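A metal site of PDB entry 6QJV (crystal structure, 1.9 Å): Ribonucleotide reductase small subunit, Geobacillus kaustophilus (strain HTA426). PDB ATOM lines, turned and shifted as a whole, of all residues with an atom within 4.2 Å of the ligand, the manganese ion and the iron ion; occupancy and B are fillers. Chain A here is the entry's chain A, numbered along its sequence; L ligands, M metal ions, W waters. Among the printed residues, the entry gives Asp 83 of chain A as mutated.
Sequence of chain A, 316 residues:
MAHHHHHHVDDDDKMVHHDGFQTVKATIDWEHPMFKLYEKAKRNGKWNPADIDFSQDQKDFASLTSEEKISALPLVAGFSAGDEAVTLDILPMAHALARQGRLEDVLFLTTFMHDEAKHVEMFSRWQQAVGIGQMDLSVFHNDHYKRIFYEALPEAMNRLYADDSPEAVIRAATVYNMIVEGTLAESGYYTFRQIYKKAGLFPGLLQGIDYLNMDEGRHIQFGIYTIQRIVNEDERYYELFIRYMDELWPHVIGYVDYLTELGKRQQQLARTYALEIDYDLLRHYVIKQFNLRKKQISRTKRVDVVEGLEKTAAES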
ATOM      1  N   LEU A  75     -23.217  28.359  18.852  1.00  0.00           N
ATOM      2  CA  LEU A  75     -22.058  27.478  18.823  1.00  0.00           C
ATOM      3  C   LEU A  75     -21.016  27.993  17.837  1.00  0.00           C
ATOM      4  O   LEU A  75     -19.815  27.931  18.112  1.00  0.00           O
ATOM      5  CB  LEU A  75     -22.497  26.066  18.447  1.00  0.00           C
ATOM      6  CG  LEU A  75     -21.586  24.879  18.744  1.00  0.00           C
ATOM      7  CD1 LEU A  75     -21.378  24.700  20.256  1.00  0.00           C
ATOM      8  CD2 LEU A  75     -22.175  23.592  18.097  1.00  0.00           C
ATOM      9  N   GLY A  78     -19.225  30.839  19.462  1.00  0.00           N
ATOM     10  CA  GLY A  78     -18.215  30.408  20.403  1.00  0.00           C
ATOM     11  C   GLY A  78     -16.945  29.940  19.710  1.00  0.00           C
ATOM     12  O   GLY A  78     -15.838  30.244  20.158  1.00  0.00           O
ATOM     13  N   PHE A  79     -17.088  29.212  18.600  1.00  0.00           N
ATOM     14  CA  PHE A  79     -15.922  28.719  17.893  1.00  0.00           C
ATOM     15  C   PHE A  79     -15.172  29.809  17.162  1.00  0.00           C
ATOM     16  O   PHE A  79     -13.945  29.817  17.174  1.00  0.00           O
ATOM     17  CB  PHE A  79     -16.302  27.606  16.927  1.00  0.00           C
ATOM     18  CG  PHE A  79     -16.146  26.231  17.511  1.00  0.00           C
ATOM     19  CD1 PHE A  79     -14.880  25.680  17.651  1.00  0.00           C
ATOM     20  CD2 PHE A  79     -17.250  25.492  17.932  1.00  0.00           C
ATOM     21  CE1 PHE A  79     -14.717  24.414  18.218  1.00  0.00           C
ATOM     22  CE2 PHE A  79     -17.068  24.217  18.488  1.00  0.00           C
ATOM     23  CZ  PHE A  79     -15.808  23.701  18.640  1.00  0.00           C
ATOM     24  N   GLY A  82     -13.299  31.747  19.558  1.00  0.00           N
ATOM     25  CA  GLY A  82     -12.323  30.896  20.223  1.00  0.00           C
ATOM     26  C   GLY A  82     -11.117  30.608  19.335  1.00  0.00           C
ATOM     27  O   GLY A  82      -9.959  30.707  19.769  1.00  0.00           O
ATOM     28  N   ASP A  83     -11.368  30.283  18.065  1.00  0.00           N
ATOM     29  CA  ASP A  83     -10.271  30.039  17.144  1.00  0.00           C
ATOM     30  C   ASP A  83      -9.475  31.310  16.871  1.00  0.00           C
ATOM     31  O   ASP A  83      -8.242  31.264  16.736  1.00  0.00           O
ATOM     32  CB  ASP A  83     -10.795  29.405  15.866  1.00  0.00           C
ATOM     33  CG  ASP A  83     -10.786  27.881  15.955  1.00  0.00           C
ATOM     34  OD1 ASP A  83      -9.709  27.339  16.216  1.00  0.00           O
ATOM     35  OD2 ASP A  83     -11.826  27.229  15.810  1.00  0.00           O
ATOM     36  N   VAL A  86      -7.219  31.804  20.059  1.00  0.00           N
ATOM     37  CA  VAL A  86      -6.057  30.908  20.168  1.00  0.00           C
ATOM     38  C   VAL A  86      -5.042  31.145  19.052  1.00  0.00           C
ATOM     39  O   VAL A  86      -3.849  30.897  19.247  1.00  0.00           O
ATOM     40  CB  VAL A  86      -6.486  29.422  20.240  1.00  0.00           C
ATOM     41  CG1 VAL A  86      -7.322  29.171  21.476  1.00  0.00           C
ATOM     42  CG2 VAL A  86      -7.223  28.966  19.023  1.00  0.00           C
ATOM     43  N   PHE A 112       1.033  24.233  14.705  1.00  0.00           N
ATOM     44  CA  PHE A 112      -0.065  24.558  15.623  1.00  0.00           C
ATOM     45  C   PHE A 112      -0.708  25.885  15.225  1.00  0.00           C
ATOM     46  O   PHE A 112      -1.936  25.997  15.065  1.00  0.00           O
ATOM     47  CB  PHE A 112       0.511  24.601  17.053  1.00  0.00           C
ATOM     48  CG  PHE A 112      -0.477  24.503  18.189  1.00  0.00           C
ATOM     49  CD1 PHE A 112      -0.111  23.857  19.364  1.00  0.00           C
ATOM     50  CD2 PHE A 112      -1.720  25.109  18.158  1.00  0.00           C
ATOM     51  CE1 PHE A 112      -0.973  23.757  20.433  1.00  0.00           C
ATOM     52  CE2 PHE A 112      -2.584  25.033  19.248  1.00  0.00           C
ATOM     53  CZ  PHE A 112      -2.187  24.372  20.399  1.00  0.00           C
ATOM     54  N   GLU A 116      -4.521  26.813  13.501  1.00  0.00           N
ATOM     55  CA  GLU A 116      -5.553  27.673  14.071  1.00  0.00           C
ATOM     56  C   GLU A 116      -5.950  28.762  13.090  1.00  0.00           C
ATOM     57  O   GLU A 116      -7.111  29.155  13.044  1.00  0.00           O
ATOM     58  CB  GLU A 116      -5.072  28.298  15.372  1.00  0.00           C
ATOM     59  CG  GLU A 116      -4.657  27.313  16.517  1.00  0.00           C
ATOM     60  CD  GLU A 116      -5.830  26.462  17.046  1.00  0.00           C
ATOM     61  OE1 GLU A 116      -5.668  25.751  18.056  1.00  0.00           O
ATOM     62  OE2 GLU A 116      -6.923  26.526  16.486  1.00  0.00           O
ATOM     63  N   HIS A 119      -8.468  27.306  11.022  1.00  0.00           N
ATOM     64  CA  HIS A 119      -9.732  27.166  11.747  1.00  0.00           C
ATOM     65  C   HIS A 119     -10.535  28.460  11.705  1.00  0.00           C
ATOM     66  O   HIS A 119     -11.748  28.447  11.460  1.00  0.00           O
ATOM     67  CB  HIS A 119      -9.469  26.751  13.190  1.00  0.00           C
ATOM     68  CG  HIS A 119      -8.817  25.416  13.304  1.00  0.00           C
ATOM     69  ND1 HIS A 119      -8.480  24.857  14.521  1.00  0.00           N
ATOM     70  CD2 HIS A 119      -8.410  24.542  12.354  1.00  0.00           C
ATOM     71  CE1 HIS A 119      -7.905  23.675  14.302  1.00  0.00           C
ATOM     72  NE2 HIS A 119      -7.837  23.476  12.996  1.00  0.00           N
ATOM     73  N   PHE A 149     -12.240  33.415  27.459  1.00  0.00           N
ATOM     74  CA  PHE A 149     -11.641  33.741  26.162  1.00  0.00           C
ATOM     75  C   PHE A 149     -11.198  35.190  26.022  1.00  0.00           C
ATOM     76  O   PHE A 149     -10.211  35.464  25.323  1.00  0.00           O
ATOM     77  CB  PHE A 149     -12.631  33.402  25.046  1.00  0.00           C
ATOM     78  CG  PHE A 149     -12.741  31.910  24.787  1.00  0.00           C
ATOM     79  CD1 PHE A 149     -11.829  31.288  23.932  1.00  0.00           C
ATOM     80  CD2 PHE A 149     -13.713  31.139  25.415  1.00  0.00           C
ATOM     81  CE1 PHE A 149     -11.884  29.950  23.710  1.00  0.00           C
ATOM     82  CE2 PHE A 149     -13.775  29.764  25.187  1.00  0.00           C
ATOM     83  CZ  PHE A 149     -12.858  29.189  24.316  1.00  0.00           C
ATOM     84  N   VAL A 180      -9.564  25.122  27.106  1.00  0.00           N
ATOM     85  CA  VAL A 180     -10.151  25.671  25.895  1.00  0.00           C
ATOM     86  C   VAL A 180     -10.263  24.586  24.804  1.00  0.00           C
ATOM     87  O   VAL A 180     -11.314  24.430  24.166  1.00  0.00           O
ATOM     88  CB  VAL A 180      -9.334  26.898  25.419  1.00  0.00           C
ATOM     89  CG1 VAL A 180      -9.582  27.233  23.974  1.00  0.00           C
ATOM     90  CG2 VAL A 180      -9.657  28.092  26.305  1.00  0.00           C
ATOM     91  N   GLU A 181      -9.183  23.864  24.536  1.00  0.00           N
ATOM     92  CA  GLU A 181      -9.148  22.817  23.515  1.00  0.00           C
ATOM     93  C   GLU A 181      -9.646  21.478  24.057  1.00  0.00           C
ATOM     94  O   GLU A 181     -10.563  20.874  23.485  1.00  0.00           O
ATOM     95  CB  GLU A 181      -7.739  22.662  22.952  1.00  0.00           C
ATOM     96  CG  GLU A 181      -7.167  23.934  22.295  1.00  0.00           C
ATOM     97  CD  GLU A 181      -5.791  23.764  21.742  1.00  0.00           C
ATOM     98  OE1 GLU A 181      -4.933  23.272  22.498  1.00  0.00           O
ATOM     99  OE2 GLU A 181      -5.583  24.105  20.544  1.00  0.00           O
ATOM    100  N   LEU A 184     -13.507  22.331  26.150  1.00  0.00           N
ATOM    101  CA  LEU A 184     -14.566  23.029  25.413  1.00  0.00           C
ATOM    102  C   LEU A 184     -14.574  22.679  23.923  1.00  0.00           C
ATOM    103  O   LEU A 184     -15.621  22.347  23.371  1.00  0.00           O
ATOM    104  CB  LEU A 184     -14.421  24.545  25.613  1.00  0.00           C
ATOM    105  CG  LEU A 184     -14.788  25.081  26.990  1.00  0.00           C
ATOM    106  CD1 LEU A 184     -14.430  26.574  27.086  1.00  0.00           C
ATOM    107  CD2 LEU A 184     -16.235  24.897  27.288  1.00  0.00           C
ATOM    108  N   ALA A 185     -13.426  22.768  23.240  1.00  0.00           N
ATOM    109  CA  ALA A 185     -13.430  22.502  21.797  1.00  0.00           C
ATOM    110  C   ALA A 185     -13.906  21.066  21.495  1.00  0.00           C
ATOM    111  O   ALA A 185     -14.718  20.839  20.581  1.00  0.00           O
ATOM    112  CB  ALA A 185     -12.043  22.715  21.203  1.00  0.00           C
ATOM    113  N   SER A 187     -15.783  19.104  23.228  1.00  0.00           N
ATOM    114  CA  SER A 187     -17.208  18.984  23.477  1.00  0.00           C
ATOM    115  C   SER A 187     -18.001  19.705  22.400  1.00  0.00           C
ATOM    116  O   SER A 187     -19.066  19.222  22.002  1.00  0.00           O
ATOM    117  CB  SER A 187     -17.558  19.534  24.863  1.00  0.00           C
ATOM    118  OG  SER A 187     -16.824  18.856  25.879  1.00  0.00           O
ATOM    119  N   GLY A 188     -17.461  20.788  21.867  1.00  0.00           N
ATOM    120  CA  GLY A 188     -18.111  21.464  20.756  1.00  0.00           C
ATOM    121  C   GLY A 188     -18.169  20.631  19.492  1.00  0.00           C
ATOM    122  O   GLY A 188     -19.197  20.625  18.794  1.00  0.00           O
ATOM    123  N   THR A 191     -20.759  18.071  20.017  1.00  0.00           N
ATOM    124  CA  THR A 191     -22.103  18.653  19.958  1.00  0.00           C
ATOM    125  C   THR A 191     -22.546  18.868  18.517  1.00  0.00           C
ATOM    126  O   THR A 191     -23.656  18.499  18.143  1.00  0.00           O
ATOM    127  CB  THR A 191     -22.128  19.962  20.755  1.00  0.00           C
ATOM    128  OG1 THR A 191     -21.859  19.684  22.130  1.00  0.00           O
ATOM    129  CG2 THR A 191     -23.466  20.661  20.700  1.00  0.00           C
ATOM    130  N   GLU A 216      -6.916  18.986  16.334  1.00  0.00           N
ATOM    131  CA  GLU A 216      -7.002  19.253  17.763  1.00  0.00           C
ATOM    132  C   GLU A 216      -6.304  18.193  18.567  1.00  0.00           C
ATOM    133  O   GLU A 216      -5.771  18.485  19.637  1.00  0.00           O
ATOM    134  CB  GLU A 216      -8.458  19.300  18.259  1.00  0.00           C
ATOM    135  CG  GLU A 216      -8.652  20.059  19.546  1.00  0.00           C
ATOM    136  CD  GLU A 216      -8.471  21.529  19.251  1.00  0.00           C
ATOM    137  OE1 GLU A 216      -9.414  22.108  18.665  1.00  0.00           O
ATOM    138  OE2 GLU A 216      -7.374  22.038  19.546  1.00  0.00           O
ATOM    139  N   HIS A 219      -2.850  19.365  19.111  1.00  0.00           N
ATOM    140  CA  HIS A 219      -2.814  20.491  20.039  1.00  0.00           C
ATOM    141  C   HIS A 219      -2.898  20.014  21.484  1.00  0.00           C
ATOM    142  O   HIS A 219      -2.141  20.466  22.367  1.00  0.00           O
ATOM    143  CB  HIS A 219      -3.958  21.475  19.708  1.00  0.00           C
ATOM    144  CG  HIS A 219      -3.965  21.943  18.287  1.00  0.00           C
ATOM    145  ND1 HIS A 219      -4.946  22.766  17.772  1.00  0.00           N
ATOM    146  CD2 HIS A 219      -3.113  21.684  17.265  1.00  0.00           C
ATOM    147  CE1 HIS A 219      -4.677  23.005  16.493  1.00  0.00           C
ATOM    148  NE2 HIS A 219      -3.575  22.346  16.162  1.00  0.00           N
ATOM    149  N   TYR A 255     -20.748  28.526  31.015  1.00  0.00           N
ATOM    150  CA  TYR A 255     -20.998  28.700  29.590  1.00  0.00           C
ATOM    151  C   TYR A 255     -21.843  27.547  29.057  1.00  0.00           C
ATOM    152  O   TYR A 255     -22.767  27.763  28.266  1.00  0.00           O
ATOM    153  CB  TYR A 255     -19.677  28.833  28.852  1.00  0.00           C
ATOM    154  CG  TYR A 255     -19.799  28.941  27.349  1.00  0.00           C
ATOM    155  CD1 TYR A 255     -20.529  29.968  26.763  1.00  0.00           C
ATOM    156  CD2 TYR A 255     -19.164  28.034  26.520  1.00  0.00           C
ATOM    157  CE1 TYR A 255     -20.613  30.068  25.352  1.00  0.00           C
ATOM    158  CE2 TYR A 255     -19.262  28.132  25.114  1.00  0.00           C
ATOM    159  CZ  TYR A 255     -19.974  29.157  24.552  1.00  0.00           C
ATOM    160  OH  TYR A 255     -20.038  29.236  23.152  1.00  0.00           O
ATOM    161  N   VAL A 256     -21.548  26.305  29.464  1.00  0.00           N
ATOM    162  CA  VAL A 256     -22.299  25.165  28.958  1.00  0.00           C
ATOM    163  C   VAL A 256     -23.777  25.309  29.347  1.00  0.00           C
ATOM    164  O   VAL A 256     -24.670  25.147  28.510  1.00  0.00           O
ATOM    165  CB  VAL A 256     -21.693  23.846  29.458  1.00  0.00           C
ATOM    166  CG1 VAL A 256     -22.618  22.646  29.172  1.00  0.00           C
ATOM    167  CG2 VAL A 256     -20.345  23.582  28.833  1.00  0.00           C
ATOM    168  N   LEU A 259     -25.473  27.928  27.059  1.00  0.00           N
ATOM    169  CA  LEU A 259     -25.808  27.394  25.742  1.00  0.00           C
ATOM    170  C   LEU A 259     -26.959  26.406  25.836  1.00  0.00           C
ATOM    171  O   LEU A 259     -27.780  26.288  24.923  1.00  0.00           O
ATOM    172  CB  LEU A 259     -24.617  26.683  25.125  1.00  0.00           C
ATOM    173  CG  LEU A 259     -23.438  27.571  24.752  1.00  0.00           C
ATOM    174  CD1 LEU A 259     -22.378  26.680  24.187  1.00  0.00           C
ATOM    175  CD2 LEU A 259     -23.847  28.628  23.734  1.00  0.00           C
ATOM    176  N   LEU A 282     -25.054  15.934  26.668  1.00  0.00           N
ATOM    177  CA  LEU A 282     -23.972  16.835  26.288  1.00  0.00           C
ATOM    178  C   LEU A 282     -23.253  17.349  27.528  1.00  0.00           C
ATOM    179  O   LEU A 282     -22.018  17.440  27.559  1.00  0.00           O
ATOM    180  CB  LEU A 282     -24.506  17.993  25.455  1.00  0.00           C
ATOM    181  CG  LEU A 282     -25.170  17.631  24.117  1.00  0.00           C
ATOM    182  CD1 LEU A 282     -25.816  18.857  23.479  1.00  0.00           C
ATOM    183  CD2 LEU A 282     -24.187  16.976  23.145  1.00  0.00           C
HETATM  184  C1  LIG L   1      -9.043  25.843  19.307  1.00  0.00           C
HETATM  185  O1  LIG L   1      -7.978  25.207  19.670  1.00  0.00           O
HETATM  186  O2  LIG L   1      -9.395  26.166  18.154  1.00  0.00           O
HETATM  187  C2  LIG L   1     -10.004  26.301  20.462  1.00  0.00           C
HETATM  188  C3  LIG L   1     -11.445  26.523  20.080  1.00  0.00           C
HETATM  189  C4  LIG L   1     -12.314  26.932  21.207  1.00  0.00           C
HETATM  190  C5  LIG L   1     -13.781  26.737  20.916  1.00  0.00           C
HETATM  191  C6  LIG L   1     -14.664  27.326  21.970  1.00  0.00           C
HETATM  192  C7  LIG L   1     -16.150  27.198  21.667  1.00  0.00           C
HETATM  193  C8  LIG L   1     -16.590  25.812  21.790  1.00  0.00           C
HETATM  194  C9  LIG L   1     -18.042  25.654  22.136  1.00  0.00           C
HETATM  195  C10 LIG L   1     -18.237  24.818  23.413  1.00  0.00           C
HETATM  196  C11 LIG L   1     -19.452  23.977  23.342  1.00  0.00           C
HETATM  197  C12 LIG L   1     -19.645  23.062  24.550  1.00  0.00           C
HETATM  198  C13 LIG L   1     -20.913  22.212  24.421  1.00  0.00           C
HETATM  199  C14 LIG L   1     -22.133  22.757  25.141  1.00  0.00           C
HETATM  200  C15 LIG L   1     -23.414  21.908  24.960  1.00  0.00           C
HETATM  201  C16 LIG L   1     -24.611  22.677  24.314  1.00  0.00           C
HETATM  202 MN    MN M   1      -8.806  25.534  16.585  1.00  0.00          MN
HETATM  203 FE    FE M   2      -6.542  23.979  18.788  1.00  0.00          FE
HETATM  204  O   HOH W   1     -10.958  24.782  16.542  1.00  0.00           O
HETATM  205  O   HOH W   2      -7.979  23.835  17.476  1.00  0.00           O
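Leu 75 touches the ligand. Gly 78 touches the ligand (O to C7, 3.4 Å). Phe 79 touches the ligand (CD1 to C5, 3.6 Å). CG2 of Val 86 touches C1 of the ligand (3.6 Å). CZ of Phe 149 touches C6 of the ligand, at 3.5 Å. Val 180 touches the ligand (CG1 to C2, 3.7 Å). O of Leu 184 touches C10 of the ligand (3.6 Å). CA of Gly 188 touches C11 of the ligand, at 3.8 Å. Thr 191 touches the ligand (OG1 to C13, 3.5 Å). Tyr 255 touches the ligand (CE2 to C10, 3.9 Å). Hydrophobic or aromatic side chains within 4 Å of the ligand: Leu 75, Phe 79, Val 86, Phe 149, Val 180 and Tyr 255. 15 residues have an atom within 4 Å of the ligand: Leu 75, Gly 78, Phe 79, Asp 83, Val 86, Glu 116, His 119, Phe 149, Val 180, Glu 181, Leu 184, Gly 188, Thr 191, Glu 216 and Tyr 255. Along chain A the residues within 4 Å of the ligand span positions 75 to 255.
The manganese ion is bound by O2 of the ligand (1.8 Å), OD1 of Asp 83 (2.1 Å), water W2 (2.1 Å), OE2 of Glu 116 (2.1 Å), ND1 of His 119 (2.2 Å) and water W1 (2.3 Å). The manganese ion has six donor atoms within binding distance.
OG1 of Thr 191 lies within hydrogen-bond range of O of Ser 187 (2.8 Å). The backbone NH (N) of Ala 185 lies within hydrogen-bond range of the backbone carbonyl oxygen (O) of Val 180 (2.8 Å).
Within 4 Å of the iron ion: Glu 116, Glu 181, Glu 216 and His 219. The nearest printed residue that does not touch the iron ion is Phe 112 (4.1 Å).
Within 4 Å of the manganese ion: Asp 83, Glu 116 and His 119. The nearest printed residue that does not touch the manganese ion is Glu 216 (4.1 Å).
The iron ion is bound by water W2 (2.0 Å), OE2 of Glu 181 (2.0 Å), O1 of the ligand (2.1 Å), OE1 of Glu 116 (2.1 Å), OE2 of Glu 216 (2.2 Å) and ND1 of His 219 (2.2 Å). The iron ion has six donor atoms within binding distance.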
